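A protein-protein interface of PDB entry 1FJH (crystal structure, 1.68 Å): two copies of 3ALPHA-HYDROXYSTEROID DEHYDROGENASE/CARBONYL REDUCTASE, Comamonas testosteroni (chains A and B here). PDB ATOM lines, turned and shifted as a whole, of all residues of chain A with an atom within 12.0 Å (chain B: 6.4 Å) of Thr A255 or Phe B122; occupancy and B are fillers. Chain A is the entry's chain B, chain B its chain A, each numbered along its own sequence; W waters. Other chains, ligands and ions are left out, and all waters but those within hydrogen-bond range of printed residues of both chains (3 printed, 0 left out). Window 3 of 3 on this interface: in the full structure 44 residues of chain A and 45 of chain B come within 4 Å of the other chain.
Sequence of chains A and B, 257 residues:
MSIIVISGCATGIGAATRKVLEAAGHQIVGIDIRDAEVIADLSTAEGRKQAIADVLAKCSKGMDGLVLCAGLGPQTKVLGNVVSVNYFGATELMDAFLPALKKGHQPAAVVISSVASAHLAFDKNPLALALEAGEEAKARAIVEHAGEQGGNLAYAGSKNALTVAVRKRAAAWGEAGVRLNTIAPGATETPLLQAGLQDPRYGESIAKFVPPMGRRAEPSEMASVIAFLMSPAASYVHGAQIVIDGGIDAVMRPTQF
Printed residues of chain B within 4 Å of Arg A253: Arg B167 (2.8 Å).
Of the printed residues of chain A, Ser B117 touches Phe A257 (3.6 Å).
No residue of chain A comes within 4 Å of Ala B121.
Phe B122 touches just one residue of chain A: Thr A255.
Asp B123 touches none of the printed residues of chain A.
Lys B124 touches none of the printed residues of chain A.
No residue of chain A comes within 4 Å of Asn B125.
No residue of chain A comes within 4 Å of Ala B128.
No residue of chain A comes within 4 Å of Leu B129.
Asn B160 touches just one residue of chain A: Phe A257.
Ala B161 touches none of the printed residues of chain A.
Val B164 touches just these residues of chain A: Pro A254 (3.9 Å) and Phe A257 (3.9 Å).
Of chain A, only Asp A249, Ala A250, Arg A253, Pro A254, Gln A256 and Phe A257 come within 4 Å of Arg B167.
Of the printed residues of chain A, Lys B168 touches Pro A254.
The nearest residue of chain B that does not touch Thr A255 is Val B164 (4.1 Å).
The nearest residue of chain A that does not touch Phe B122 is Phe A257 (6.3 Å).
NE of Arg B167 lies within hydrogen-bond range of O of Pro A254, 3.1 Å away.
O of Gln A256 lies within hydrogen-bond range of NH2 of Arg B167 (3.1 Å).
The guanidinium group of Arg B167 is in hydrogen-bond range of the backbone carbonyl oxygen of Arg A253, at 2.8 Å.
The side-chain carboxylate of Asp A249 is in salt-bridge range of the guanidinium group of Arg B167, at 2.9 Å.
Printed residues of chain B that touch a printed residue of chain A: Ser B117, Phe B122, Asn B160, Val B164, Arg B167 and Lys B168.
Hydrophobic or aromatic side chains of chain B within 4 Å of the printed part of chain A: Phe B122 and Val B164.
Of the 13 printed residues of chain A, 7 touch a printed residue of chain B.
Hydrophobic or aromatic side chains of chain A within 4 Å of the printed part of chain B: Ala A250, Pro A254 and Phe A257.
Among the printed residues, 12 pairs touch across the chains.
Among the printed residues, Asp or Glu carboxylates within 4 Å of a Lys or Arg side-chain nitrogen of the other chain: Asp A249 with Arg B167 (2.9 Å).
OD1 of Asp A249 lies within salt-bridge range of NE of Arg A253 (2.9 Å).
OE1 of Glu B132 is in salt-bridge range of NZ of Lys B168.
The guanidinium group of Arg A253 is in hydrogen-bond range of the side-chain amide oxygen of Gln A256, at 2.7 Å.
The backbone carbonyl oxygen of Leu B120 sits close to the side-chain amide oxygen of Asn B160 (2.9 Å).
The side-chain amide nitrogen (ND2) of Asn B125 lies close to the side-chain amide nitrogen (ND2) of Asn B160 (3.0 Å).
The backbone carbonyl oxygen of Ser B117 sits close to the side-chain amide oxygen of Asn B160 (2.9 Å).
NH2 of Arg B167 touches CA of Ala A250, at 3.7 Å.
Val B164 touches Pro A254 (CG2 to O, 3.9 Å).
Lys B168 touches Pro A254.
Thr A255 touches Phe B122 (CG2 to CD1, 3.7 Å).
Ser B117 touches Phe A257 (O to CE1, 3.6 Å).
Asn B160 touches Phe A257 (OD1 to CZ, 3.8 Å).
Val B164 touches Phe A257.
Arg B167 touches Phe A257 (CD to CD2, 3.7 Å).
No position is printed for both chains.
Of the 12 pairs that touch across the chains among the printed residues, none has its exchanged pair printed and touching as well.
Water W3 lies within hydrogen-bond range of the side-chain carboxylate of Asp A249 (2.7 Å), the guanidinium group of Arg A253 (2.8 Å), the backbone carbonyl oxygen of Gln A256 (2.8 Å) and the guanidinium group of Arg B167 (3.2 Å).
Water W1 bridges OD2 of Asp A249 (2.7 Å) and NH1 of Arg B167 (3.0 Å).
Water W2 lies within hydrogen-bond range of the backbone carbonyl oxygen of Thr A255 (2.8 Å), the backbone NH of Phe B122 (2.9 Å) and the side-chain amide oxygen of Asn B160 (3.2 Å).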
ATOM      1  N   ALA A 118     -13.681  25.587   6.179  1.00  0.00           N
ATOM      2  CA  ALA A 118     -14.150  24.663   5.155  1.00  0.00           C
ATOM      3  C   ALA A 118     -15.672  24.582   5.096  1.00  0.00           C
ATOM      4  O   ALA A 118     -16.224  23.818   4.301  1.00  0.00           O
ATOM      5  CB  ALA A 118     -13.561  23.279   5.399  1.00  0.00           C
ATOM      6  N   VAL A 243      -5.538  19.993  10.178  1.00  0.00           N
ATOM      7  CA  VAL A 243      -6.787  19.930  10.927  1.00  0.00           C
ATOM      8  C   VAL A 243      -6.570  19.194  12.249  1.00  0.00           C
ATOM      9  O   VAL A 243      -6.058  18.080  12.270  1.00  0.00           O
ATOM     10  CB  VAL A 243      -7.886  19.193  10.120  1.00  0.00           C
ATOM     11  CG1 VAL A 243      -9.177  19.139  10.929  1.00  0.00           C
ATOM     12  CG2 VAL A 243      -8.125  19.900   8.785  1.00  0.00           C
ATOM     13  N   GLY A 247     -11.175  14.153  14.507  1.00  0.00           N
ATOM     14  CA  GLY A 247     -11.842  13.372  13.474  1.00  0.00           C
ATOM     15  C   GLY A 247     -13.157  13.870  12.909  1.00  0.00           C
ATOM     16  O   GLY A 247     -13.675  13.290  11.952  1.00  0.00           O
ATOM     17  N   ILE A 248     -13.696  14.944  13.473  1.00  0.00           N
ATOM     18  CA  ILE A 248     -14.973  15.480  13.009  1.00  0.00           C
ATOM     19  C   ILE A 248     -15.025  15.778  11.515  1.00  0.00           C
ATOM     20  O   ILE A 248     -15.957  15.357  10.821  1.00  0.00           O
ATOM     21  CB  ILE A 248     -15.342  16.771  13.781  1.00  0.00           C
ATOM     22  CG1 ILE A 248     -15.631  16.432  15.243  1.00  0.00           C
ATOM     23  CG2 ILE A 248     -16.558  17.440  13.141  1.00  0.00           C
ATOM     24  CD1 ILE A 248     -16.853  15.562  15.440  1.00  0.00           C
ATOM     25  N   ASP A 249     -14.033  16.511  11.020  1.00  0.00           N
ATOM     26  CA  ASP A 249     -13.985  16.875   9.610  1.00  0.00           C
ATOM     27  C   ASP A 249     -14.000  15.647   8.698  1.00  0.00           C
ATOM     28  O   ASP A 249     -14.660  15.641   7.653  1.00  0.00           O
ATOM     29  CB  ASP A 249     -12.740  17.721   9.342  1.00  0.00           C
ATOM     30  CG  ASP A 249     -12.667  18.215   7.918  1.00  0.00           C
ATOM     31  OD1 ASP A 249     -13.559  18.991   7.513  1.00  0.00           O
ATOM     32  OD2 ASP A 249     -11.720  17.827   7.204  1.00  0.00           O
ATOM     33  N   ALA A 250     -13.281  14.603   9.098  1.00  0.00           N
ATOM     34  CA  ALA A 250     -13.232  13.375   8.312  1.00  0.00           C
ATOM     35  C   ALA A 250     -14.619  12.739   8.221  1.00  0.00           C
ATOM     36  O   ALA A 250     -15.004  12.222   7.174  1.00  0.00           O
ATOM     37  CB  ALA A 250     -12.244  12.395   8.935  1.00  0.00           C
ATOM     38  N   VAL A 251     -15.369  12.786   9.319  1.00  0.00           N
ATOM     39  CA  VAL A 251     -16.709  12.205   9.351  1.00  0.00           C
ATOM     40  C   VAL A 251     -17.706  13.029   8.535  1.00  0.00           C
ATOM     41  O   VAL A 251     -18.532  12.474   7.805  1.00  0.00           O
ATOM     42  CB  VAL A 251     -17.233  12.078  10.809  1.00  0.00           C
ATOM     43  CG1 VAL A 251     -18.694  11.637  10.806  1.00  0.00           C
ATOM     44  CG2 VAL A 251     -16.398  11.068  11.576  1.00  0.00           C
ATOM     45  N   MET A 252     -17.619  14.352   8.651  1.00  0.00           N
ATOM     46  CA  MET A 252     -18.517  15.258   7.936  1.00  0.00           C
ATOM     47  C   MET A 252     -18.198  15.408   6.443  1.00  0.00           C
ATOM     48  O   MET A 252     -19.107  15.497   5.615  1.00  0.00           O
ATOM     49  CB  MET A 252     -18.486  16.646   8.583  1.00  0.00           C
ATOM     50  CG  MET A 252     -18.831  16.673  10.065  1.00  0.00           C
ATOM     51  SD  MET A 252     -20.557  16.287  10.401  1.00  0.00           S
ATOM     52  CE  MET A 252     -20.465  14.534  10.690  1.00  0.00           C
ATOM     53  N   ARG A 253     -16.911  15.445   6.105  1.00  0.00           N
ATOM     54  CA  ARG A 253     -16.486  15.610   4.714  1.00  0.00           C
ATOM     55  C   ARG A 253     -15.438  14.577   4.309  1.00  0.00           C
ATOM     56  O   ARG A 253     -14.305  14.927   3.995  1.00  0.00           O
ATOM     57  CB  ARG A 253     -15.886  17.001   4.503  1.00  0.00           C
ATOM     58  CG  ARG A 253     -16.708  18.167   5.015  1.00  0.00           C
ATOM     59  CD  ARG A 253     -16.062  19.467   4.557  1.00  0.00           C
ATOM     60  NE  ARG A 253     -14.638  19.496   4.880  1.00  0.00           N
ATOM     61  CZ  ARG A 253     -13.742  20.255   4.257  1.00  0.00           C
ATOM     62  NH1 ARG A 253     -14.116  21.057   3.269  1.00  0.00           N
ATOM     63  NH2 ARG A 253     -12.468  20.207   4.616  1.00  0.00           N
ATOM     64  N   PRO A 254     -15.805  13.293   4.294  1.00  0.00           N
ATOM     65  CA  PRO A 254     -14.837  12.260   3.915  1.00  0.00           C
ATOM     66  C   PRO A 254     -14.191  12.431   2.536  1.00  0.00           C
ATOM     67  O   PRO A 254     -13.011  12.115   2.354  1.00  0.00           O
ATOM     68  CB  PRO A 254     -15.652  10.972   4.022  1.00  0.00           C
ATOM     69  CG  PRO A 254     -17.063  11.434   3.715  1.00  0.00           C
ATOM     70  CD  PRO A 254     -17.144  12.714   4.508  1.00  0.00           C
ATOM     71  N   THR A 255     -14.952  12.948   1.576  1.00  0.00           N
ATOM     72  CA  THR A 255     -14.453  13.122   0.216  1.00  0.00           C
ATOM     73  C   THR A 255     -13.880  14.501  -0.085  1.00  0.00           C
ATOM     74  O   THR A 255     -13.465  14.768  -1.212  1.00  0.00           O
ATOM     75  CB  THR A 255     -15.560  12.837  -0.819  1.00  0.00           C
ATOM     76  OG1 THR A 255     -16.568  13.853  -0.731  1.00  0.00           O
ATOM     77  CG2 THR A 255     -16.202  11.481  -0.553  1.00  0.00           C
ATOM     78  N   GLN A 256     -13.853  15.379   0.908  1.00  0.00           N
ATOM     79  CA  GLN A 256     -13.327  16.719   0.687  1.00  0.00           C
ATOM     80  C   GLN A 256     -12.088  16.990   1.529  1.00  0.00           C
ATOM     81  O   GLN A 256     -12.128  16.931   2.754  1.00  0.00           O
ATOM     82  CB  GLN A 256     -14.408  17.761   0.982  1.00  0.00           C
ATOM     83  CG  GLN A 256     -14.042  19.175   0.560  1.00  0.00           C
ATOM     84  CD  GLN A 256     -15.250  20.094   0.500  1.00  0.00           C
ATOM     85  OE1 GLN A 256     -15.944  20.294   1.497  1.00  0.00           O
ATOM     86  NE2 GLN A 256     -15.507  20.656  -0.676  1.00  0.00           N
ATOM     87  N   PHE A 257     -10.985  17.288   0.848  1.00  0.00           N
ATOM     88  CA  PHE A 257      -9.707  17.561   1.492  1.00  0.00           C
ATOM     89  C   PHE A 257      -8.782  18.240   0.489  1.00  0.00           C
ATOM     90  O   PHE A 257      -9.283  18.635  -0.584  1.00  0.00           O
ATOM     91  CB  PHE A 257      -9.090  16.249   1.990  1.00  0.00           C
ATOM     92  CG  PHE A 257      -9.107  15.146   0.965  1.00  0.00           C
ATOM     93  CD1 PHE A 257      -8.192  15.134  -0.082  1.00  0.00           C
ATOM     94  CD2 PHE A 257     -10.067  14.143   1.026  1.00  0.00           C
ATOM     95  CE1 PHE A 257      -8.235  14.136  -1.058  1.00  0.00           C
ATOM     96  CE2 PHE A 257     -10.119  13.143   0.058  1.00  0.00           C
ATOM     97  CZ  PHE A 257      -9.202  13.141  -0.984  1.00  0.00           C
ATOM     98  OXT PHE A 257      -7.576  18.382   0.776  1.00  0.00           O
ATOM     99  N   SER B 117      -3.881  12.490  -4.582  1.00  0.00           N
ATOM    100  CA  SER B 117      -5.198  12.102  -4.095  1.00  0.00           C
ATOM    101  C   SER B 117      -6.198  13.240  -4.280  1.00  0.00           C
ATOM    102  O   SER B 117      -7.403  13.009  -4.362  1.00  0.00           O
ATOM    103  CB  SER B 117      -5.121  11.741  -2.615  1.00  0.00           C
ATOM    104  OG  SER B 117      -4.688  12.859  -1.866  1.00  0.00           O
ATOM    105  N   LEU B 120      -8.184  14.482  -8.237  1.00  0.00           N
ATOM    106  CA  LEU B 120      -9.370  13.837  -8.786  1.00  0.00           C
ATOM    107  C   LEU B 120     -10.441  13.819  -7.698  1.00  0.00           C
ATOM    108  O   LEU B 120     -10.139  13.545  -6.540  1.00  0.00           O
ATOM    109  CB  LEU B 120      -9.018  12.400  -9.195  1.00  0.00           C
ATOM    110  CG  LEU B 120      -9.983  11.551 -10.024  1.00  0.00           C
ATOM    111  CD1 LEU B 120      -9.952  12.000 -11.480  1.00  0.00           C
ATOM    112  CD2 LEU B 120      -9.574  10.091  -9.930  1.00  0.00           C
ATOM    113  N   ALA B 121     -11.683  14.125  -8.060  1.00  0.00           N
ATOM    114  CA  ALA B 121     -12.774  14.117  -7.093  1.00  0.00           C
ATOM    115  C   ALA B 121     -13.265  12.679  -6.922  1.00  0.00           C
ATOM    116  O   ALA B 121     -13.377  11.942  -7.897  1.00  0.00           O
ATOM    117  CB  ALA B 121     -13.910  15.011  -7.577  1.00  0.00           C
ATOM    118  N   PHE B 122     -13.551  12.280  -5.685  1.00  0.00           N
ATOM    119  CA  PHE B 122     -14.011  10.922  -5.419  1.00  0.00           C
ATOM    120  C   PHE B 122     -15.255  10.562  -6.232  1.00  0.00           C
ATOM    121  O   PHE B 122     -15.375   9.443  -6.736  1.00  0.00           O
ATOM    122  CB  PHE B 122     -14.298  10.744  -3.923  1.00  0.00           C
ATOM    123  CG  PHE B 122     -14.595   9.325  -3.527  1.00  0.00           C
ATOM    124  CD1 PHE B 122     -15.903   8.915  -3.269  1.00  0.00           C
ATOM    125  CD2 PHE B 122     -13.566   8.392  -3.412  1.00  0.00           C
ATOM    126  CE1 PHE B 122     -16.178   7.599  -2.900  1.00  0.00           C
ATOM    127  CE2 PHE B 122     -13.834   7.073  -3.045  1.00  0.00           C
ATOM    128  CZ  PHE B 122     -15.143   6.678  -2.789  1.00  0.00           C
ATOM    129  N   ASP B 123     -16.174  11.512  -6.363  1.00  0.00           N
ATOM    130  CA  ASP B 123     -17.404  11.277  -7.111  1.00  0.00           C
ATOM    131  C   ASP B 123     -17.170  11.183  -8.617  1.00  0.00           C
ATOM    132  O   ASP B 123     -18.072  10.809  -9.367  1.00  0.00           O
ATOM    133  CB  ASP B 123     -18.424  12.383  -6.814  1.00  0.00           C
ATOM    134  CG  ASP B 123     -17.922  13.764  -7.195  1.00  0.00           C
ATOM    135  OD1 ASP B 123     -18.672  14.744  -7.001  1.00  0.00           O
ATOM    136  OD2 ASP B 123     -16.779  13.875  -7.686  1.00  0.00           O
ATOM    137  N   LYS B 124     -15.961  11.520  -9.053  1.00  0.00           N
ATOM    138  CA  LYS B 124     -15.605  11.472 -10.469  1.00  0.00           C
ATOM    139  C   LYS B 124     -14.435  10.515 -10.687  1.00  0.00           C
ATOM    140  O   LYS B 124     -13.821  10.501 -11.753  1.00  0.00           O
ATOM    141  CB  LYS B 124     -15.223  12.872 -10.960  1.00  0.00           C
ATOM    142  CG  LYS B 124     -16.341  13.901 -10.830  1.00  0.00           C
ATOM    143  CD  LYS B 124     -17.464  13.620 -11.814  1.00  0.00           C
ATOM    144  CE  LYS B 124     -18.828  13.717 -11.150  1.00  0.00           C
ATOM    145  NZ  LYS B 124     -19.018  15.003 -10.440  1.00  0.00           N
ATOM    146  N   ASN B 125     -14.137   9.720  -9.665  1.00  0.00           N
ATOM    147  CA  ASN B 125     -13.043   8.750  -9.707  1.00  0.00           C
ATOM    148  C   ASN B 125     -13.552   7.426 -10.278  1.00  0.00           C
ATOM    149  O   ASN B 125     -14.264   6.687  -9.606  1.00  0.00           O
ATOM    150  CB  ASN B 125     -12.506   8.534  -8.287  1.00  0.00           C
ATOM    151  CG  ASN B 125     -11.313   7.596  -8.241  1.00  0.00           C
ATOM    152  OD1 ASN B 125     -11.031   6.877  -9.202  1.00  0.00           O
ATOM    153  ND2 ASN B 125     -10.617   7.583  -7.104  1.00  0.00           N
ATOM    154  N   PRO B 126     -13.177   7.105 -11.528  1.00  0.00           N
ATOM    155  CA  PRO B 126     -13.613   5.862 -12.174  1.00  0.00           C
ATOM    156  C   PRO B 126     -13.311   4.570 -11.417  1.00  0.00           C
ATOM    157  O   PRO B 126     -13.870   3.521 -11.735  1.00  0.00           O
ATOM    158  CB  PRO B 126     -12.928   5.921 -13.542  1.00  0.00           C
ATOM    159  CG  PRO B 126     -11.715   6.741 -13.283  1.00  0.00           C
ATOM    160  CD  PRO B 126     -12.233   7.836 -12.388  1.00  0.00           C
ATOM    161  N   ALA B 128     -13.355   4.553  -7.869  1.00  0.00           N
ATOM    162  CA  ALA B 128     -14.051   4.680  -6.589  1.00  0.00           C
ATOM    163  C   ALA B 128     -15.002   3.550  -6.195  1.00  0.00           C
ATOM    164  O   ALA B 128     -14.765   2.855  -5.208  1.00  0.00           O
ATOM    165  CB  ALA B 128     -14.789   6.016  -6.537  1.00  0.00           C
ATOM    166  N   LEU B 129     -16.082   3.374  -6.949  1.00  0.00           N
ATOM    167  CA  LEU B 129     -17.060   2.337  -6.632  1.00  0.00           C
ATOM    168  C   LEU B 129     -16.472   0.932  -6.569  1.00  0.00           C
ATOM    169  O   LEU B 129     -16.730   0.193  -5.619  1.00  0.00           O
ATOM    170  CB  LEU B 129     -18.221   2.369  -7.632  1.00  0.00           C
ATOM    171  CG  LEU B 129     -19.296   3.445  -7.420  1.00  0.00           C
ATOM    172  CD1 LEU B 129     -19.962   3.238  -6.066  1.00  0.00           C
ATOM    173  CD2 LEU B 129     -18.680   4.831  -7.498  1.00  0.00           C
ATOM    174  N   GLU B 132     -14.228   0.609  -3.426  1.00  0.00           N
ATOM    175  CA  GLU B 132     -15.060   0.580  -2.227  1.00  0.00           C
ATOM    176  C   GLU B 132     -15.787  -0.753  -2.107  1.00  0.00           C
ATOM    177  O   GLU B 132     -15.942  -1.291  -1.012  1.00  0.00           O
ATOM    178  CB  GLU B 132     -16.093   1.711  -2.255  1.00  0.00           C
ATOM    179  CG  GLU B 132     -15.768   2.856  -1.318  1.00  0.00           C
ATOM    180  CD  GLU B 132     -16.891   3.871  -1.195  1.00  0.00           C
ATOM    181  OE1 GLU B 132     -16.764   4.783  -0.354  1.00  0.00           O
ATOM    182  OE2 GLU B 132     -17.895   3.764  -1.931  1.00  0.00           O
ATOM    183  N   ASN B 160      -6.582   8.654  -4.343  1.00  0.00           N
ATOM    184  CA  ASN B 160      -7.778   9.406  -3.984  1.00  0.00           C
ATOM    185  C   ASN B 160      -8.718   8.495  -3.195  1.00  0.00           C
ATOM    186  O   ASN B 160      -9.223   8.870  -2.137  1.00  0.00           O
ATOM    187  CB  ASN B 160      -8.514   9.913  -5.227  1.00  0.00           C
ATOM    188  CG  ASN B 160      -9.860  10.526  -4.884  1.00  0.00           C
ATOM    189  OD1 ASN B 160      -9.937  11.650  -4.382  1.00  0.00           O
ATOM    190  ND2 ASN B 160     -10.927   9.777  -5.128  1.00  0.00           N
ATOM    191  N   ALA B 161      -8.949   7.295  -3.719  1.00  0.00           N
ATOM    192  CA  ALA B 161      -9.823   6.338  -3.060  1.00  0.00           C
ATOM    193  C   ALA B 161      -9.265   5.954  -1.694  1.00  0.00           C
ATOM    194  O   ALA B 161     -10.021   5.717  -0.755  1.00  0.00           O
ATOM    195  CB  ALA B 161      -9.991   5.090  -3.935  1.00  0.00           C
ATOM    196  N   LEU B 162      -7.937   5.907  -1.589  1.00  0.00           N
ATOM    197  CA  LEU B 162      -7.274   5.544  -0.342  1.00  0.00           C
ATOM    198  C   LEU B 162      -7.535   6.586   0.736  1.00  0.00           C
ATOM    199  O   LEU B 162      -7.907   6.243   1.861  1.00  0.00           O
ATOM    200  CB  LEU B 162      -5.761   5.417  -0.556  1.00  0.00           C
ATOM    201  CG  LEU B 162      -4.978   4.324   0.185  1.00  0.00           C
ATOM    202  CD1 LEU B 162      -3.553   4.809   0.399  1.00  0.00           C
ATOM    203  CD2 LEU B 162      -5.628   3.966   1.505  1.00  0.00           C
ATOM    204  N   VAL B 164      -9.944   8.688   0.910  1.00  0.00           N
ATOM    205  CA  VAL B 164     -11.358   8.655   1.275  1.00  0.00           C
ATOM    206  C   VAL B 164     -11.644   7.452   2.173  1.00  0.00           C
ATOM    207  O   VAL B 164     -12.399   7.553   3.141  1.00  0.00           O
ATOM    208  CB  VAL B 164     -12.257   8.588   0.020  1.00  0.00           C
ATOM    209  CG1 VAL B 164     -13.714   8.311   0.421  1.00  0.00           C
ATOM    210  CG2 VAL B 164     -12.157   9.904  -0.741  1.00  0.00           C
ATOM    211  N   ALA B 165     -11.026   6.317   1.857  1.00  0.00           N
ATOM    212  CA  ALA B 165     -11.214   5.108   2.648  1.00  0.00           C
ATOM    213  C   ALA B 165     -10.765   5.345   4.084  1.00  0.00           C
ATOM    214  O   ALA B 165     -11.426   4.920   5.030  1.00  0.00           O
ATOM    215  CB  ALA B 165     -10.429   3.952   2.040  1.00  0.00           C
ATOM    216  N   ARG B 167     -10.570   8.264   5.624  1.00  0.00           N
ATOM    217  CA  ARG B 167     -11.455   9.226   6.270  1.00  0.00           C
ATOM    218  C   ARG B 167     -12.793   8.613   6.677  1.00  0.00           C
ATOM    219  O   ARG B 167     -13.354   8.972   7.713  1.00  0.00           O
ATOM    220  CB  ARG B 167     -11.647  10.451   5.367  1.00  0.00           C
ATOM    221  CG  ARG B 167     -10.387  11.331   5.317  1.00  0.00           C
ATOM    222  CD  ARG B 167     -10.443  12.403   4.232  1.00  0.00           C
ATOM    223  NE  ARG B 167     -11.357  13.516   4.501  1.00  0.00           N
ATOM    224  CZ  ARG B 167     -11.153  14.473   5.407  1.00  0.00           C
ATOM    225  NH1 ARG B 167     -10.063  14.466   6.164  1.00  0.00           N
ATOM    226  NH2 ARG B 167     -12.029  15.462   5.531  1.00  0.00           N
ATOM    227  N   LYS B 168     -13.295   7.669   5.885  1.00  0.00           N
ATOM    228  CA  LYS B 168     -14.559   7.017   6.214  1.00  0.00           C
ATOM    229  C   LYS B 168     -14.414   6.054   7.393  1.00  0.00           C
ATOM    230  O   LYS B 168     -15.408   5.575   7.944  1.00  0.00           O
ATOM    231  CB  LYS B 168     -15.109   6.269   4.993  1.00  0.00           C
ATOM    232  CG  LYS B 168     -15.594   7.193   3.890  1.00  0.00           C
ATOM    233  CD  LYS B 168     -16.354   6.428   2.805  1.00  0.00           C
ATOM    234  CE  LYS B 168     -16.874   7.375   1.733  1.00  0.00           C
ATOM    235  NZ  LYS B 168     -17.806   6.691   0.789  1.00  0.00           N
HETATM  236  O   HOH W   1      -9.619  16.523   8.260  1.00  0.00           O
HETATM  237  O   HOH W   2     -12.307  13.500  -3.372  1.00  0.00           O
HETATM  238  O   HOH W   3     -10.586  18.169   4.794  1.00  0.00           O
